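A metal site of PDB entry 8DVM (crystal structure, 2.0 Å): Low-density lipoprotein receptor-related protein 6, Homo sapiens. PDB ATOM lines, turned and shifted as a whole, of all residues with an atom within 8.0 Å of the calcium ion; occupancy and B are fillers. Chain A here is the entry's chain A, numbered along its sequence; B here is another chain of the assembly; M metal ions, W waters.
Water W3 bridges OD1 of Asp 119 (2.6 Å) and ND2 of Asn 98 (3.3 Å).
NZ of Lys 7 of chain B is in hydrogen-bond range of OG1 of Thr 95.
The backbone carbonyl oxygen of Tyr 77 sits at hydrogen-bond distance from the backbone NH of Thr 95 (3.0 Å).
The side-chain carboxylate (OE2) of Glu 79 lies within hydrogen-bond range of the side-chain hydroxyl (OG1) of Thr 95, 2.6 Å away.
The backbone carbonyl oxygen (O) of Ser 120 is in hydrogen-bond range of the backbone NH (N) of Trp 138.
The backbone carbonyl oxygen of Leu 118 sits close to the side-chain amide nitrogen of Asn 98 (3.3 Å).
Within 4 Å of the calcium ion: Thr 95, Asn 98 and Ser 120.
The calcium ion is bound by water W3 (2.4 Å), water W1 (2.5 Å), the backbone carbonyl oxygen of Thr 95 (2.6 Å), water W2 (2.6 Å), the side-chain hydroxyl of Ser 120 (2.7 Å) and the side-chain amide oxygen of Asn 98 (2.7 Å).
The calcium ion has six donor atoms within binding distance.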
ATOM      1  N   ASP A  76      21.392 -12.228 -20.607  1.00  0.00           N
ATOM      2  CA  ASP A  76      21.902 -13.589 -20.623  1.00  0.00           C
ATOM      3  C   ASP A  76      20.774 -14.613 -20.755  1.00  0.00           C
ATOM      4  O   ASP A  76      20.716 -15.340 -21.738  1.00  0.00           O
ATOM      5  CB  ASP A  76      22.712 -13.839 -19.348  1.00  0.00           C
ATOM      6  CG  ASP A  76      23.563 -15.089 -19.405  1.00  0.00           C
ATOM      7  OD1 ASP A  76      23.708 -15.705 -20.484  1.00  0.00           O
ATOM      8  OD2 ASP A  76      24.053 -15.468 -18.319  1.00  0.00           O
ATOM      9  N   TYR A  77      19.849 -14.645 -19.793  1.00  0.00           N
ATOM     10  CA  TYR A  77      18.687 -15.527 -19.841  1.00  0.00           C
ATOM     11  C   TYR A  77      17.478 -14.646 -19.554  1.00  0.00           C
ATOM     12  O   TYR A  77      16.959 -14.618 -18.420  1.00  0.00           O
ATOM     13  CB  TYR A  77      18.813 -16.676 -18.849  1.00  0.00           C
ATOM     14  CG  TYR A  77      19.855 -17.702 -19.234  1.00  0.00           C
ATOM     15  CD1 TYR A  77      21.186 -17.518 -18.906  1.00  0.00           C
ATOM     16  CD2 TYR A  77      19.500 -18.857 -19.914  1.00  0.00           C
ATOM     17  CE1 TYR A  77      22.156 -18.454 -19.248  1.00  0.00           C
ATOM     18  CE2 TYR A  77      20.465 -19.810 -20.270  1.00  0.00           C
ATOM     19  CZ  TYR A  77      21.781 -19.600 -19.924  1.00  0.00           C
ATOM     20  OH  TYR A  77      22.737 -20.526 -20.281  1.00  0.00           O
ATOM     21  N   GLU A  79      14.294 -14.514 -19.137  1.00  0.00           N
ATOM     22  CA  GLU A  79      13.177 -15.449 -19.021  1.00  0.00           C
ATOM     23  C   GLU A  79      11.853 -14.806 -18.614  1.00  0.00           C
ATOM     24  O   GLU A  79      10.821 -15.492 -18.650  1.00  0.00           O
ATOM     25  CB  GLU A  79      13.556 -16.557 -18.034  1.00  0.00           C
ATOM     26  CG  GLU A  79      14.796 -17.339 -18.495  1.00  0.00           C
ATOM     27  CD  GLU A  79      15.201 -18.486 -17.578  1.00  0.00           C
ATOM     28  OE1 GLU A  79      14.313 -19.254 -17.123  1.00  0.00           O
ATOM     29  OE2 GLU A  79      16.428 -18.650 -17.339  1.00  0.00           O
ATOM     30  N   ASP A  94      16.168 -11.178 -15.769  1.00  0.00           N
ATOM     31  CA  ASP A  94      17.178 -12.045 -16.358  1.00  0.00           C
ATOM     32  C   ASP A  94      17.776 -12.948 -15.292  1.00  0.00           C
ATOM     33  O   ASP A  94      18.357 -12.451 -14.328  1.00  0.00           O
ATOM     34  CB  ASP A  94      18.280 -11.220 -17.027  1.00  0.00           C
ATOM     35  CG  ASP A  94      19.105 -12.043 -18.018  1.00  0.00           C
ATOM     36  OD1 ASP A  94      19.882 -12.916 -17.558  1.00  0.00           O
ATOM     37  OD2 ASP A  94      19.005 -11.808 -19.254  1.00  0.00           O
ATOM     38  N   THR A  95      17.667 -14.273 -15.503  1.00  0.00           N
ATOM     39  CA  THR A  95      18.207 -15.242 -14.551  1.00  0.00           C
ATOM     40  C   THR A  95      19.706 -15.396 -14.668  1.00  0.00           C
ATOM     41  O   THR A  95      20.313 -16.061 -13.828  1.00  0.00           O
ATOM     42  CB  THR A  95      17.598 -16.662 -14.716  1.00  0.00           C
ATOM     43  OG1 THR A  95      18.157 -17.293 -15.871  1.00  0.00           O
ATOM     44  CG2 THR A  95      16.090 -16.659 -14.786  1.00  0.00           C
ATOM     45  N   GLY A  96      20.308 -14.869 -15.727  1.00  0.00           N
ATOM     46  CA  GLY A  96      21.749 -14.901 -15.857  1.00  0.00           C
ATOM     47  C   GLY A  96      22.392 -13.694 -15.201  1.00  0.00           C
ATOM     48  O   GLY A  96      23.258 -13.854 -14.327  1.00  0.00           O
ATOM     49  N   THR A  97      21.981 -12.498 -15.601  1.00  0.00           N
ATOM     50  CA  THR A  97      22.530 -11.286 -15.012  1.00  0.00           C
ATOM     51  C   THR A  97      21.964 -10.973 -13.627  1.00  0.00           C
ATOM     52  O   THR A  97      22.508 -10.086 -12.958  1.00  0.00           O
ATOM     53  CB  THR A  97      22.285 -10.090 -15.929  1.00  0.00           C
ATOM     54  OG1 THR A  97      20.882  -9.840 -16.003  1.00  0.00           O
ATOM     55  CG2 THR A  97      22.826 -10.359 -17.310  1.00  0.00           C
ATOM     56  N   ASN A  98      20.899 -11.642 -13.190  1.00  0.00           N
ATOM     57  CA  ASN A  98      20.280 -11.363 -11.881  1.00  0.00           C
ATOM     58  C   ASN A  98      19.844  -9.901 -11.775  1.00  0.00           C
ATOM     59  O   ASN A  98      20.154  -9.199 -10.803  1.00  0.00           O
ATOM     60  CB  ASN A  98      21.219 -11.719 -10.737  1.00  0.00           C
ATOM     61  CG  ASN A  98      21.327 -13.196 -10.541  1.00  0.00           C
ATOM     62  OD1 ASN A  98      20.513 -13.961 -11.058  1.00  0.00           O
ATOM     63  ND2 ASN A  98      22.337 -13.620  -9.783  1.00  0.00           N
ATOM     64  N   ARG A  99      19.088  -9.453 -12.776  1.00  0.00           N
ATOM     65  CA  ARG A  99      18.627  -8.072 -12.837  1.00  0.00           C
ATOM     66  C   ARG A  99      17.167  -8.039 -13.241  1.00  0.00           C
ATOM     67  O   ARG A  99      16.693  -8.893 -13.987  1.00  0.00           O
ATOM     68  CB  ARG A  99      19.476  -7.249 -13.819  1.00  0.00           C
ATOM     69  CG  ARG A  99      20.826  -6.783 -13.258  1.00  0.00           C
ATOM     70  CD  ARG A  99      21.659  -6.102 -14.322  1.00  0.00           C
ATOM     71  NE  ARG A  99      23.049  -5.957 -13.910  1.00  0.00           N
ATOM     72  CZ  ARG A  99      23.855  -4.998 -14.338  1.00  0.00           C
ATOM     73  NH1 ARG A  99      23.432  -4.060 -15.161  1.00  0.00           N
ATOM     74  NH2 ARG A  99      25.126  -4.986 -13.940  1.00  0.00           N
ATOM     75  N   LEU A 118      19.546 -10.521  -5.570  1.00  0.00           N
ATOM     76  CA  LEU A 118      18.548 -10.983  -6.522  1.00  0.00           C
ATOM     77  C   LEU A 118      19.097 -12.262  -7.140  1.00  0.00           C
ATOM     78  O   LEU A 118      20.108 -12.223  -7.852  1.00  0.00           O
ATOM     79  CB  LEU A 118      18.276  -9.928  -7.589  1.00  0.00           C
ATOM     80  CG  LEU A 118      16.974 -10.048  -8.385  1.00  0.00           C
ATOM     81  CD1 LEU A 118      15.770 -10.123  -7.449  1.00  0.00           C
ATOM     82  CD2 LEU A 118      16.859  -8.856  -9.304  1.00  0.00           C
ATOM     83  N   ASP A 119      18.448 -13.385  -6.845  1.00  0.00           N
ATOM     84  CA  ASP A 119      18.928 -14.705  -7.225  1.00  0.00           C
ATOM     85  C   ASP A 119      17.933 -15.330  -8.209  1.00  0.00           C
ATOM     86  O   ASP A 119      16.927 -15.915  -7.807  1.00  0.00           O
ATOM     87  CB  ASP A 119      19.126 -15.568  -5.978  1.00  0.00           C
ATOM     88  CG  ASP A 119      19.998 -16.761  -6.248  1.00  0.00           C
ATOM     89  OD1 ASP A 119      20.465 -16.931  -7.392  1.00  0.00           O
ATOM     90  OD2 ASP A 119      20.243 -17.525  -5.287  1.00  0.00           O
ATOM     91  N   SER A 120      18.256 -15.189  -9.504  1.00  0.00           N
ATOM     92  CA  SER A 120      17.527 -15.702 -10.656  1.00  0.00           C
ATOM     93  C   SER A 120      16.060 -15.270 -10.665  1.00  0.00           C
ATOM     94  O   SER A 120      15.173 -16.125 -10.529  1.00  0.00           O
ATOM     95  CB  SER A 120      17.627 -17.223 -10.714  1.00  0.00           C
ATOM     96  OG  SER A 120      18.970 -17.658 -10.559  1.00  0.00           O
ATOM     97  N   PRO A 121      15.778 -13.979 -10.835  1.00  0.00           N
ATOM     98  CA  PRO A 121      14.379 -13.556 -11.056  1.00  0.00           C
ATOM     99  C   PRO A 121      13.871 -14.119 -12.374  1.00  0.00           C
ATOM    100  O   PRO A 121      14.550 -14.011 -13.403  1.00  0.00           O
ATOM    101  CB  PRO A 121      14.469 -12.026 -11.117  1.00  0.00           C
ATOM    102  CG  PRO A 121      15.902 -11.765 -11.615  1.00  0.00           C
ATOM    103  CD  PRO A 121      16.746 -12.879 -11.051  1.00  0.00           C
ATOM    104  N   TRP A 138      14.153 -18.169  -8.783  1.00  0.00           N
ATOM    105  CA  TRP A 138      14.491 -19.587  -8.881  1.00  0.00           C
ATOM    106  C   TRP A 138      15.836 -19.906  -8.264  1.00  0.00           C
ATOM    107  O   TRP A 138      16.450 -20.908  -8.620  1.00  0.00           O
ATOM    108  CB  TRP A 138      14.523 -20.062 -10.337  1.00  0.00           C
ATOM    109  CG  TRP A 138      13.206 -20.246 -10.950  1.00  0.00           C
ATOM    110  CD1 TRP A 138      11.999 -19.880 -10.433  1.00  0.00           C
ATOM    111  CD2 TRP A 138      12.932 -20.801 -12.240  1.00  0.00           C
ATOM    112  NE1 TRP A 138      10.996 -20.178 -11.309  1.00  0.00           N
ATOM    113  CE2 TRP A 138      11.540 -20.753 -12.434  1.00  0.00           C
ATOM    114  CE3 TRP A 138      13.731 -21.359 -13.242  1.00  0.00           C
ATOM    115  CZ2 TRP A 138      10.925 -21.217 -13.592  1.00  0.00           C
ATOM    116  CZ3 TRP A 138      13.128 -21.818 -14.395  1.00  0.00           C
ATOM    117  CH2 TRP A 138      11.730 -21.741 -14.557  1.00  0.00           C
ATOM    118  N   GLY A 139      16.349 -19.043  -7.406  1.00  0.00           N
ATOM    119  CA  GLY A 139      17.703 -19.178  -6.900  1.00  0.00           C
ATOM    120  C   GLY A 139      17.718 -19.272  -5.395  1.00  0.00           C
ATOM    121  O   GLY A 139      16.943 -18.572  -4.717  1.00  0.00           O
ATOM    122  N   GLY A 140      18.612 -20.105  -4.865  1.00  0.00           N
ATOM    123  CA  GLY A 140      18.791 -20.233  -3.439  1.00  0.00           C
ATOM    124  C   GLY A 140      17.513 -20.692  -2.810  1.00  0.00           C
ATOM    125  O   GLY A 140      17.118 -21.846  -2.990  1.00  0.00           O
ATOM    126  N   LYS B   7      20.787 -24.843 -19.506  1.00  0.00           N
ATOM    127  CA  LYS B   7      20.942 -24.351 -18.148  1.00  0.00           C
ATOM    128  C   LYS B   7      20.121 -25.050 -17.081  1.00  0.00           C
ATOM    129  O   LYS B   7      20.622 -25.360 -16.017  1.00  0.00           O
ATOM    130  CB  LYS B   7      20.630 -22.859 -18.077  1.00  0.00           C
ATOM    131  CG  LYS B   7      20.725 -22.266 -16.692  1.00  0.00           C
ATOM    132  CD  LYS B   7      20.418 -20.783 -16.685  1.00  0.00           C
ATOM    133  CE  LYS B   7      20.650 -20.192 -15.322  1.00  0.00           C
ATOM    134  NZ  LYS B   7      20.690 -18.706 -15.341  1.00  0.00           N
ATOM    135  N   TRP B   8      18.865 -25.312 -17.375  1.00  0.00           N
ATOM    136  CA  TRP B   8      17.988 -25.838 -16.348  1.00  0.00           C
ATOM    137  C   TRP B   8      17.629 -27.339 -16.433  1.00  0.00           C
ATOM    138  O   TRP B   8      16.989 -27.870 -15.550  1.00  0.00           O
ATOM    139  CB  TRP B   8      16.711 -25.002 -16.284  1.00  0.00           C
ATOM    140  CG  TRP B   8      16.861 -23.544 -16.047  1.00  0.00           C
ATOM    141  CD1 TRP B   8      16.768 -22.553 -16.974  1.00  0.00           C
ATOM    142  CD2 TRP B   8      17.063 -22.901 -14.788  1.00  0.00           C
ATOM    143  NE1 TRP B   8      16.934 -21.334 -16.373  1.00  0.00           N
ATOM    144  CE2 TRP B   8      17.121 -21.523 -15.035  1.00  0.00           C
ATOM    145  CE3 TRP B   8      17.234 -23.356 -13.488  1.00  0.00           C
ATOM    146  CZ2 TRP B   8      17.325 -20.600 -14.022  1.00  0.00           C
ATOM    147  CZ3 TRP B   8      17.438 -22.442 -12.487  1.00  0.00           C
ATOM    148  CH2 TRP B   8      17.486 -21.075 -12.760  1.00  0.00           C
HETATM  149 CA    CA M   1      21.242 -16.554 -11.493  1.00  0.00          CA
HETATM  150  O   HOH W   1      23.448 -15.885 -12.422  1.00  0.00           O
HETATM  151  O   HOH W   2      21.567 -18.877 -12.538  1.00  0.00           O
HETATM  152  O   HOH W   3      22.137 -16.850  -9.328  1.00  0.00           O
